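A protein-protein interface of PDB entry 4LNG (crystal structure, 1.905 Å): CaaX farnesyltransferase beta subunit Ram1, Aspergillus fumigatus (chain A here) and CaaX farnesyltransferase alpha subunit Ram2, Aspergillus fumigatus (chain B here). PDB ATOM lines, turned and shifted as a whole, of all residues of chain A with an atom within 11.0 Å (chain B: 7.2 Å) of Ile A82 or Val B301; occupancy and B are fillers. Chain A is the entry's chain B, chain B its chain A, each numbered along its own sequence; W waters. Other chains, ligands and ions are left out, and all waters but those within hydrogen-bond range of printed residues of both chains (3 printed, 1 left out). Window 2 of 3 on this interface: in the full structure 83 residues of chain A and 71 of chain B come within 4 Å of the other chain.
Of chain B, only Glu B257, Val B301, Lys B302 and Tyr B338 come within 4 Å of Ile A82.
No residue of chain A comes within 4 Å of Ala B300.
Printed residues of chain A within 4 Å of Tyr B338: Ile A82.
Printed residues of chain B within 4 Å of Asp A84: Pro B256 (3.4 Å) and Glu B257 (3.1 Å).
Printed residues of chain B within 4 Å of Leu A81: Lys B337 (3.7 Å).
Of the printed residues of chain A, Pro B256 touches Asp A84.
The nearest residue of chain B that does not touch Ile A82 is Ser B303 (4.5 Å).
OD2 of Asp A84 is in hydrogen-bond range of N of Glu B257, at 3.1 Å.
O of Glu B257 sits at hydrogen-bond distance from NE2 of His B305 (2.7 Å).
OH of Tyr B338 sits at hydrogen-bond distance from NZ of Lys B337.
The backbone carbonyl oxygen (O) of Phe B286 is in hydrogen-bond range of the backbone NH (N) of Lys B302, 2.9 Å away.
The backbone NH (N) of Tyr B338 is in hydrogen-bond range of the backbone carbonyl oxygen (O) of Leu B333, 3.0 Å away.
O of Pro B256 lies within hydrogen-bond range of OG of Ser B303, at 2.8 Å.
The side-chain carboxylate of Glu B257 lies within hydrogen-bond range of the side-chain hydroxyl of Ser B304 (2.8 Å).
Of the 15 printed residues of chain B, 6 touch a printed residue of chain A.
Hydrophobic or aromatic side chains of chain B that line the printed part of chain A: Pro B256 and Tyr B338.
Hydrophobic or aromatic side chains of chain A that line the printed part of chain B: Leu A81 and Ile A82.
Among the printed residues, merely in contact across the chains: Ile A82 with Val B301, Asp A84 with Pro B256, Ile A82 with Glu B257, Leu A81 with Lys B337, Ile A82 with Lys B302 and Ile A82 with Tyr B338.
Water W1 lies within hydrogen-bond range of OD1 of Asn A361 (2.8 Å) and O of Glu B257 (3.4 Å).
Water W2 bridges the backbone NH of Leu A81 (3.1 Å) and the backbone carbonyl oxygen of Lys B337 (3.4 Å).
Water W3 bridges N of Ile A82 (3.1 Å) and O of Tyr B338 (3.2 Å).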
ATOM      1  N   LEU A  75     -27.053 -14.944 -17.037  1.00  0.00           N
ATOM      2  CA  LEU A  75     -25.730 -14.441 -17.398  1.00  0.00           C
ATOM      3  C   LEU A  75     -25.720 -13.781 -18.776  1.00  0.00           C
ATOM      4  O   LEU A  75     -24.961 -12.842 -19.021  1.00  0.00           O
ATOM      5  CB  LEU A  75     -24.709 -15.584 -17.358  1.00  0.00           C
ATOM      6  CG  LEU A  75     -23.269 -15.254 -17.746  1.00  0.00           C
ATOM      7  CD1 LEU A  75     -22.733 -14.155 -16.845  1.00  0.00           C
ATOM      8  CD2 LEU A  75     -22.392 -16.498 -17.670  1.00  0.00           C
ATOM      9  N   GLU A  78     -28.559 -10.061 -19.061  1.00  0.00           N
ATOM     10  CA  GLU A  78     -28.432  -8.872 -18.226  1.00  0.00           C
ATOM     11  C   GLU A  78     -27.031  -8.289 -18.339  1.00  0.00           C
ATOM     12  O   GLU A  78     -26.075  -9.020 -18.590  1.00  0.00           O
ATOM     13  CB  GLU A  78     -28.700  -9.223 -16.758  1.00  0.00           C
ATOM     14  CG  GLU A  78     -30.066  -9.817 -16.477  1.00  0.00           C
ATOM     15  CD  GLU A  78     -30.165 -10.408 -15.083  1.00  0.00           C
ATOM     16  OE1 GLU A  78     -29.158 -10.367 -14.344  1.00  0.00           O
ATOM     17  OE2 GLU A  78     -31.248 -10.917 -14.729  1.00  0.00           O
ATOM     18  N   PRO A  79     -26.902  -6.966 -18.144  1.00  0.00           N
ATOM     19  CA  PRO A  79     -25.578  -6.340 -18.073  1.00  0.00           C
ATOM     20  C   PRO A  79     -24.838  -6.818 -16.821  1.00  0.00           C
ATOM     21  O   PRO A  79     -25.477  -7.373 -15.927  1.00  0.00           O
ATOM     22  CB  PRO A  79     -25.903  -4.844 -17.958  1.00  0.00           C
ATOM     23  CG  PRO A  79     -27.321  -4.709 -18.438  1.00  0.00           C
ATOM     24  CD  PRO A  79     -27.988  -5.979 -18.023  1.00  0.00           C
ATOM     25  N   PRO A  80     -23.510  -6.616 -16.757  1.00  0.00           N
ATOM     26  CA  PRO A  80     -22.729  -7.007 -15.573  1.00  0.00           C
ATOM     27  C   PRO A  80     -23.237  -6.349 -14.286  1.00  0.00           C
ATOM     28  O   PRO A  80     -23.866  -5.294 -14.346  1.00  0.00           O
ATOM     29  CB  PRO A  80     -21.321  -6.499 -15.902  1.00  0.00           C
ATOM     30  CG  PRO A  80     -21.272  -6.465 -17.394  1.00  0.00           C
ATOM     31  CD  PRO A  80     -22.654  -6.086 -17.835  1.00  0.00           C
ATOM     32  N   LEU A  81     -22.968  -6.973 -13.142  1.00  0.00           N
ATOM     33  CA  LEU A  81     -23.416  -6.455 -11.849  1.00  0.00           C
ATOM     34  C   LEU A  81     -22.700  -5.167 -11.452  1.00  0.00           C
ATOM     35  O   LEU A  81     -23.335  -4.195 -11.037  1.00  0.00           O
ATOM     36  CB  LEU A  81     -23.212  -7.501 -10.750  1.00  0.00           C
ATOM     37  CG  LEU A  81     -24.124  -8.726 -10.729  1.00  0.00           C
ATOM     38  CD1 LEU A  81     -23.732  -9.650  -9.584  1.00  0.00           C
ATOM     39  CD2 LEU A  81     -25.581  -8.312 -10.606  1.00  0.00           C
ATOM     40  N   ILE A  82     -21.375  -5.168 -11.571  1.00  0.00           N
ATOM     41  CA  ILE A  82     -20.570  -4.022 -11.155  1.00  0.00           C
ATOM     42  C   ILE A  82     -20.605  -2.913 -12.199  1.00  0.00           C
ATOM     43  O   ILE A  82     -20.295  -3.141 -13.369  1.00  0.00           O
ATOM     44  CB  ILE A  82     -19.100  -4.415 -10.896  1.00  0.00           C
ATOM     45  CG1 ILE A  82     -19.016  -5.608  -9.943  1.00  0.00           C
ATOM     46  CG2 ILE A  82     -18.316  -3.226 -10.345  1.00  0.00           C
ATOM     47  CD1 ILE A  82     -19.734  -5.396  -8.644  1.00  0.00           C
ATOM     48  N   HIS A  83     -21.001  -1.717 -11.782  1.00  0.00           N
ATOM     49  CA  HIS A  83     -21.033  -0.579 -12.692  1.00  0.00           C
ATOM     50  C   HIS A  83     -20.455   0.682 -12.061  1.00  0.00           C
ATOM     51  O   HIS A  83     -20.927   1.152 -11.025  1.00  0.00           O
ATOM     52  CB  HIS A  83     -22.453  -0.329 -13.211  1.00  0.00           C
ATOM     53  CG  HIS A  83     -22.757  -1.040 -14.495  1.00  0.00           C
ATOM     54  ND1 HIS A  83     -23.189  -2.348 -14.539  1.00  0.00           N
ATOM     55  CD2 HIS A  83     -22.681  -0.626 -15.782  1.00  0.00           C
ATOM     56  CE1 HIS A  83     -23.371  -2.707 -15.798  1.00  0.00           C
ATOM     57  NE2 HIS A  83     -23.071  -1.681 -16.572  1.00  0.00           N
ATOM     58  N   ASP A  84     -19.420   1.218 -12.699  1.00  0.00           N
ATOM     59  CA  ASP A  84     -18.770   2.445 -12.246  1.00  0.00           C
ATOM     60  C   ASP A  84     -19.636   3.658 -12.575  1.00  0.00           C
ATOM     61  O   ASP A  84     -20.353   3.663 -13.575  1.00  0.00           O
ATOM     62  CB  ASP A  84     -17.402   2.612 -12.912  1.00  0.00           C
ATOM     63  CG  ASP A  84     -16.372   1.615 -12.408  1.00  0.00           C
ATOM     64  OD1 ASP A  84     -16.497   1.150 -11.256  1.00  0.00           O
ATOM     65  OD2 ASP A  84     -15.429   1.310 -13.167  1.00  0.00           O
ATOM     66  N   LEU A  85     -19.554   4.690 -11.741  1.00  0.00           N
ATOM     67  CA  LEU A  85     -20.312   5.917 -11.963  1.00  0.00           C
ATOM     68  C   LEU A  85     -19.735   6.744 -13.108  1.00  0.00           C
ATOM     69  O   LEU A  85     -20.476   7.368 -13.868  1.00  0.00           O
ATOM     70  CB  LEU A  85     -20.348   6.763 -10.689  1.00  0.00           C
ATOM     71  CG  LEU A  85     -21.003   6.132  -9.461  1.00  0.00           C
ATOM     72  CD1 LEU A  85     -20.990   7.106  -8.291  1.00  0.00           C
ATOM     73  CD2 LEU A  85     -22.423   5.677  -9.778  1.00  0.00           C
ATOM     74  N   LEU A  86     -18.411   6.750 -13.222  1.00  0.00           N
ATOM     75  CA  LEU A  86     -17.728   7.537 -14.248  1.00  0.00           C
ATOM     76  C   LEU A  86     -18.035   7.055 -15.663  1.00  0.00           C
ATOM     77  O   LEU A  86     -17.831   5.887 -15.989  1.00  0.00           O
ATOM     78  CB  LEU A  86     -16.214   7.519 -14.028  1.00  0.00           C
ATOM     79  CG  LEU A  86     -15.417   8.270 -15.101  1.00  0.00           C
ATOM     80  CD1 LEU A  86     -15.769   9.749 -15.087  1.00  0.00           C
ATOM     81  CD2 LEU A  86     -13.917   8.066 -14.925  1.00  0.00           C
ATOM     82  N   THR A  91     -16.954   3.348 -21.961  1.00  0.00           N
ATOM     83  CA  THR A  91     -18.178   2.785 -21.396  1.00  0.00           C
ATOM     84  C   THR A  91     -19.397   3.080 -22.260  1.00  0.00           C
ATOM     85  O   THR A  91     -20.340   2.292 -22.297  1.00  0.00           O
ATOM     86  CB  THR A  91     -18.433   3.250 -19.943  1.00  0.00           C
ATOM     87  OG1 THR A  91     -18.476   4.679 -19.886  1.00  0.00           O
ATOM     88  CG2 THR A  91     -17.336   2.746 -19.032  1.00  0.00           C
ATOM     89  N   GLN A  94     -19.209   0.473 -24.934  1.00  0.00           N
ATOM     90  CA  GLN A  94     -19.470  -0.839 -24.347  1.00  0.00           C
ATOM     91  C   GLN A  94     -20.956  -1.005 -24.033  1.00  0.00           C
ATOM     92  O   GLN A  94     -21.538  -2.063 -24.280  1.00  0.00           O
ATOM     93  CB  GLN A  94     -18.618  -1.048 -23.089  1.00  0.00           C
ATOM     94  CG  GLN A  94     -18.911  -2.341 -22.334  1.00  0.00           C
ATOM     95  CD  GLN A  94     -18.619  -3.585 -23.156  1.00  0.00           C
ATOM     96  OE1 GLN A  94     -17.739  -3.582 -24.020  1.00  0.00           O
ATOM     97  NE2 GLN A  94     -19.359  -4.659 -22.888  1.00  0.00           N
ATOM     98  N   SER A  95     -21.561   0.047 -23.490  1.00  0.00           N
ATOM     99  CA  SER A  95     -22.985   0.043 -23.169  1.00  0.00           C
ATOM    100  C   SER A  95     -23.847  -0.136 -24.414  1.00  0.00           C
ATOM    101  O   SER A  95     -24.810  -0.906 -24.406  1.00  0.00           O
ATOM    102  CB  SER A  95     -23.374   1.337 -22.452  1.00  0.00           C
ATOM    103  OG  SER A  95     -24.762   1.364 -22.174  1.00  0.00           O
ATOM    104  N   VAL A  98     -23.580  -3.798 -25.636  1.00  0.00           N
ATOM    105  CA  VAL A  98     -24.397  -4.670 -24.800  1.00  0.00           C
ATOM    106  C   VAL A  98     -25.875  -4.518 -25.147  1.00  0.00           C
ATOM    107  O   VAL A  98     -26.594  -5.505 -25.291  1.00  0.00           O
ATOM    108  CB  VAL A  98     -24.186  -4.380 -23.301  1.00  0.00           C
ATOM    109  CG1 VAL A  98     -25.278  -5.037 -22.463  1.00  0.00           C
ATOM    110  CG2 VAL A  98     -22.808  -4.851 -22.861  1.00  0.00           C
ATOM    111  N   ALA A 351     -19.357 -11.093 -20.708  1.00  0.00           N
ATOM    112  CA  ALA A 351     -20.779 -11.388 -20.574  1.00  0.00           C
ATOM    113  C   ALA A 351     -21.488 -10.048 -20.421  1.00  0.00           C
ATOM    114  O   ALA A 351     -20.953  -9.137 -19.789  1.00  0.00           O
ATOM    115  CB  ALA A 351     -21.028 -12.265 -19.364  1.00  0.00           C
ATOM    116  N   PRO A 352     -22.708  -9.923 -20.967  1.00  0.00           N
ATOM    117  CA  PRO A 352     -23.531 -10.993 -21.542  1.00  0.00           C
ATOM    118  C   PRO A 352     -23.231 -11.340 -23.002  1.00  0.00           C
ATOM    119  O   PRO A 352     -23.792 -12.325 -23.474  1.00  0.00           O
ATOM    120  CB  PRO A 352     -24.945 -10.420 -21.432  1.00  0.00           C
ATOM    121  CG  PRO A 352     -24.741  -8.951 -21.629  1.00  0.00           C
ATOM    122  CD  PRO A 352     -23.421  -8.631 -20.957  1.00  0.00           C
ATOM    123  N   ASN A 361     -10.362  -3.414 -22.619  1.00  0.00           N
ATOM    124  CA  ASN A 361     -11.272  -2.269 -22.678  1.00  0.00           C
ATOM    125  C   ASN A 361     -11.783  -1.890 -24.071  1.00  0.00           C
ATOM    126  O   ASN A 361     -12.277  -0.781 -24.269  1.00  0.00           O
ATOM    127  CB  ASN A 361     -10.680  -1.046 -21.960  1.00  0.00           C
ATOM    128  CG  ASN A 361     -11.021  -1.019 -20.483  1.00  0.00           C
ATOM    129  OD1 ASN A 361     -12.126  -1.385 -20.085  1.00  0.00           O
ATOM    130  ND2 ASN A 361     -10.074  -0.581 -19.662  1.00  0.00           N
ATOM    131  N   PRO B 256     -13.153   1.894 -10.154  1.00  0.00           N
ATOM    132  CA  PRO B 256     -12.542   0.656  -9.653  1.00  0.00           C
ATOM    133  C   PRO B 256     -12.680  -0.563 -10.568  1.00  0.00           C
ATOM    134  O   PRO B 256     -11.833  -1.450 -10.500  1.00  0.00           O
ATOM    135  CB  PRO B 256     -13.284   0.416  -8.332  1.00  0.00           C
ATOM    136  CG  PRO B 256     -13.730   1.774  -7.908  1.00  0.00           C
ATOM    137  CD  PRO B 256     -14.099   2.469  -9.183  1.00  0.00           C
ATOM    138  N   GLU B 257     -13.716  -0.609 -11.403  1.00  0.00           N
ATOM    139  CA  GLU B 257     -13.933  -1.761 -12.277  1.00  0.00           C
ATOM    140  C   GLU B 257     -13.108  -1.678 -13.572  1.00  0.00           C
ATOM    141  O   GLU B 257     -13.110  -2.599 -14.389  1.00  0.00           O
ATOM    142  CB  GLU B 257     -15.434  -1.939 -12.563  1.00  0.00           C
ATOM    143  CG  GLU B 257     -15.829  -3.237 -13.274  1.00  0.00           C
ATOM    144  CD  GLU B 257     -15.420  -4.496 -12.519  1.00  0.00           C
ATOM    145  OE1 GLU B 257     -15.147  -4.418 -11.302  1.00  0.00           O
ATOM    146  OE2 GLU B 257     -15.374  -5.574 -13.149  1.00  0.00           O
ATOM    147  N   PHE B 286     -12.106  -2.515  -1.358  1.00  0.00           N
ATOM    148  CA  PHE B 286     -13.151  -2.582  -2.375  1.00  0.00           C
ATOM    149  C   PHE B 286     -14.094  -3.755  -2.139  1.00  0.00           C
ATOM    150  O   PHE B 286     -15.003  -3.997  -2.935  1.00  0.00           O
ATOM    151  CB  PHE B 286     -12.539  -2.673  -3.777  1.00  0.00           C
ATOM    152  CG  PHE B 286     -11.705  -1.482  -4.148  1.00  0.00           C
ATOM    153  CD1 PHE B 286     -12.297  -0.327  -4.625  1.00  0.00           C
ATOM    154  CD2 PHE B 286     -10.327  -1.515  -4.011  1.00  0.00           C
ATOM    155  CE1 PHE B 286     -11.532   0.776  -4.959  1.00  0.00           C
ATOM    156  CE2 PHE B 286      -9.557  -0.418  -4.345  1.00  0.00           C
ATOM    157  CZ  PHE B 286     -10.160   0.728  -4.820  1.00  0.00           C
ATOM    158  N   VAL B 287     -13.877  -4.477  -1.044  1.00  0.00           N
ATOM    159  CA  VAL B 287     -14.688  -5.647  -0.721  1.00  0.00           C
ATOM    160  C   VAL B 287     -15.504  -5.452   0.558  1.00  0.00           C
ATOM    161  O   VAL B 287     -15.125  -4.685   1.443  1.00  0.00           O
ATOM    162  CB  VAL B 287     -13.820  -6.910  -0.574  1.00  0.00           C
ATOM    163  CG1 VAL B 287     -14.670  -8.089  -0.126  1.00  0.00           C
ATOM    164  CG2 VAL B 287     -13.114  -7.222  -1.883  1.00  0.00           C
ATOM    165  N   ALA B 300     -20.350  -6.618  -0.435  1.00  0.00           N
ATOM    166  CA  ALA B 300     -20.247  -5.274  -0.996  1.00  0.00           C
ATOM    167  C   ALA B 300     -18.978  -5.135  -1.827  1.00  0.00           C
ATOM    168  O   ALA B 300     -17.946  -4.684  -1.330  1.00  0.00           O
ATOM    169  CB  ALA B 300     -20.271  -4.236   0.111  1.00  0.00           C
ATOM    170  N   VAL B 301     -19.060  -5.523  -3.097  1.00  0.00           N
ATOM    171  CA  VAL B 301     -17.894  -5.511  -3.976  1.00  0.00           C
ATOM    172  C   VAL B 301     -17.961  -4.393  -5.012  1.00  0.00           C
ATOM    173  O   VAL B 301     -18.915  -4.303  -5.784  1.00  0.00           O
ATOM    174  CB  VAL B 301     -17.727  -6.857  -4.698  1.00  0.00           C
ATOM    175  CG1 VAL B 301     -16.619  -6.769  -5.732  1.00  0.00           C
ATOM    176  CG2 VAL B 301     -17.445  -7.961  -3.692  1.00  0.00           C
ATOM    177  N   LYS B 302     -16.938  -3.545  -5.027  1.00  0.00           N
ATOM    178  CA  LYS B 302     -16.889  -2.425  -5.958  1.00  0.00           C
ATOM    179  C   LYS B 302     -15.909  -2.667  -7.104  1.00  0.00           C
ATOM    180  O   LYS B 302     -15.776  -1.832  -7.998  1.00  0.00           O
ATOM    181  CB  LYS B 302     -16.534  -1.134  -5.218  1.00  0.00           C
ATOM    182  CG  LYS B 302     -17.551  -0.732  -4.160  1.00  0.00           C
ATOM    183  CD  LYS B 302     -17.134   0.552  -3.460  1.00  0.00           C
ATOM    184  CE  LYS B 302     -18.186   1.006  -2.457  1.00  0.00           C
ATOM    185  NZ  LYS B 302     -18.440  -0.024  -1.410  1.00  0.00           N
ATOM    186  N   SER B 303     -15.231  -3.812  -7.076  1.00  0.00           N
ATOM    187  CA  SER B 303     -14.271  -4.162  -8.119  1.00  0.00           C
ATOM    188  C   SER B 303     -13.942  -5.652  -8.124  1.00  0.00           C
ATOM    189  O   SER B 303     -13.440  -6.186  -7.137  1.00  0.00           O
ATOM    190  CB  SER B 303     -12.979  -3.359  -7.951  1.00  0.00           C
ATOM    191  OG  SER B 303     -12.023  -3.738  -8.928  1.00  0.00           O
ATOM    192  N   SER B 304     -14.214  -6.316  -9.243  1.00  0.00           N
ATOM    193  CA  SER B 304     -13.855  -7.723  -9.395  1.00  0.00           C
ATOM    194  C   SER B 304     -12.338  -7.907  -9.486  1.00  0.00           C
ATOM    195  O   SER B 304     -11.810  -8.974  -9.162  1.00  0.00           O
ATOM    196  CB  SER B 304     -14.534  -8.319 -10.627  1.00  0.00           C
ATOM    197  OG  SER B 304     -14.095  -7.675 -11.808  1.00  0.00           O
ATOM    198  N   HIS B 305     -11.640  -6.863  -9.926  1.00  0.00           N
ATOM    199  CA  HIS B 305     -10.183  -6.908 -10.020  1.00  0.00           C
ATOM    200  C   HIS B 305      -9.554  -6.958  -8.630  1.00  0.00           C
ATOM    201  O   HIS B 305      -8.499  -7.565  -8.434  1.00  0.00           O
ATOM    202  CB  HIS B 305      -9.669  -5.702 -10.809  1.00  0.00           C
ATOM    203  CG  HIS B 305     -10.418  -5.470 -12.083  1.00  0.00           C
ATOM    204  ND1 HIS B 305     -10.370  -6.350 -13.142  1.00  0.00           N
ATOM    205  CD2 HIS B 305     -11.256  -4.475 -12.457  1.00  0.00           C
ATOM    206  CE1 HIS B 305     -11.141  -5.903 -14.117  1.00  0.00           C
ATOM    207  NE2 HIS B 305     -11.687  -4.765 -13.729  1.00  0.00           N
ATOM    208  N   ALA B 306     -10.215  -6.324  -7.668  1.00  0.00           N
ATOM    209  CA  ALA B 306      -9.787  -6.387  -6.275  1.00  0.00           C
ATOM    210  C   ALA B 306      -9.933  -7.805  -5.726  1.00  0.00           C
ATOM    211  O   ALA B 306      -9.114  -8.255  -4.928  1.00  0.00           O
ATOM    212  CB  ALA B 306     -10.577  -5.399  -5.431  1.00  0.00           C
ATOM    213  N   ILE B 307     -10.978  -8.503  -6.159  1.00  0.00           N
ATOM    214  CA  ILE B 307     -11.202  -9.886  -5.748  1.00  0.00           C
ATOM    215  C   ILE B 307     -10.134 -10.819  -6.318  1.00  0.00           C
ATOM    216  O   ILE B 307      -9.604 -11.681  -5.608  1.00  0.00           O
ATOM    217  CB  ILE B 307     -12.589 -10.394  -6.188  1.00  0.00           C
ATOM    218  CG1 ILE B 307     -13.695  -9.523  -5.594  1.00  0.00           C
ATOM    219  CG2 ILE B 307     -12.790 -11.843  -5.771  1.00  0.00           C
ATOM    220  CD1 ILE B 307     -15.080 -10.011  -5.940  1.00  0.00           C
ATOM    221  N   LEU B 333     -16.493 -16.477  -5.488  1.00  0.00           N
ATOM    222  CA  LEU B 333     -17.259 -15.250  -5.691  1.00  0.00           C
ATOM    223  C   LEU B 333     -17.181 -14.809  -7.150  1.00  0.00           C
ATOM    224  O   LEU B 333     -18.172 -14.360  -7.728  1.00  0.00           O
ATOM    225  CB  LEU B 333     -16.741 -14.130  -4.783  1.00  0.00           C
ATOM    226  CG  LEU B 333     -16.881 -14.334  -3.272  1.00  0.00           C
ATOM    227  CD1 LEU B 333     -16.160 -13.228  -2.517  1.00  0.00           C
ATOM    228  CD2 LEU B 333     -18.342 -14.379  -2.874  1.00  0.00           C
ATOM    229  N   LYS B 337     -20.611 -14.973  -9.140  1.00  0.00           N
ATOM    230  CA  LYS B 337     -21.243 -13.658  -9.154  1.00  0.00           C
ATOM    231  C   LYS B 337     -20.549 -12.603 -10.003  1.00  0.00           C
ATOM    232  O   LYS B 337     -21.171 -11.990 -10.868  1.00  0.00           O
ATOM    233  CB  LYS B 337     -21.405 -13.122  -7.730  1.00  0.00           C
ATOM    234  CG  LYS B 337     -22.575 -13.711  -6.970  1.00  0.00           C
ATOM    235  CD  LYS B 337     -22.873 -12.898  -5.718  1.00  0.00           C
ATOM    236  CE  LYS B 337     -23.157 -11.444  -6.065  1.00  0.00           C
ATOM    237  NZ  LYS B 337     -23.496 -10.637  -4.858  1.00  0.00           N
ATOM    238  N   TYR B 338     -19.265 -12.382  -9.749  1.00  0.00           N
ATOM    239  CA  TYR B 338     -18.611 -11.171 -10.244  1.00  0.00           C
ATOM    240  C   TYR B 338     -17.927 -11.261 -11.612  1.00  0.00           C
ATOM    241  O   TYR B 338     -17.743 -10.241 -12.277  1.00  0.00           O
ATOM    242  CB  TYR B 338     -17.688 -10.600  -9.169  1.00  0.00           C
ATOM    243  CG  TYR B 338     -18.468 -10.203  -7.937  1.00  0.00           C
ATOM    244  CD1 TYR B 338     -19.303  -9.094  -7.955  1.00  0.00           C
ATOM    245  CD2 TYR B 338     -18.397 -10.951  -6.770  1.00  0.00           C
ATOM    246  CE1 TYR B 338     -20.033  -8.730  -6.845  1.00  0.00           C
ATOM    247  CE2 TYR B 338     -19.123 -10.594  -5.650  1.00  0.00           C
ATOM    248  CZ  TYR B 338     -19.939  -9.481  -5.695  1.00  0.00           C
ATOM    249  OH  TYR B 338     -20.665  -9.117  -4.591  1.00  0.00           O
HETATM  250  O   HOH W   1     -12.181  -2.760 -17.614  1.00  0.00           O
HETATM  251  O   HOH W   2     -21.299  -9.574 -13.309  1.00  0.00           O
HETATM  252  O   HOH W   3     -19.616  -7.618 -12.314  1.00  0.00           O
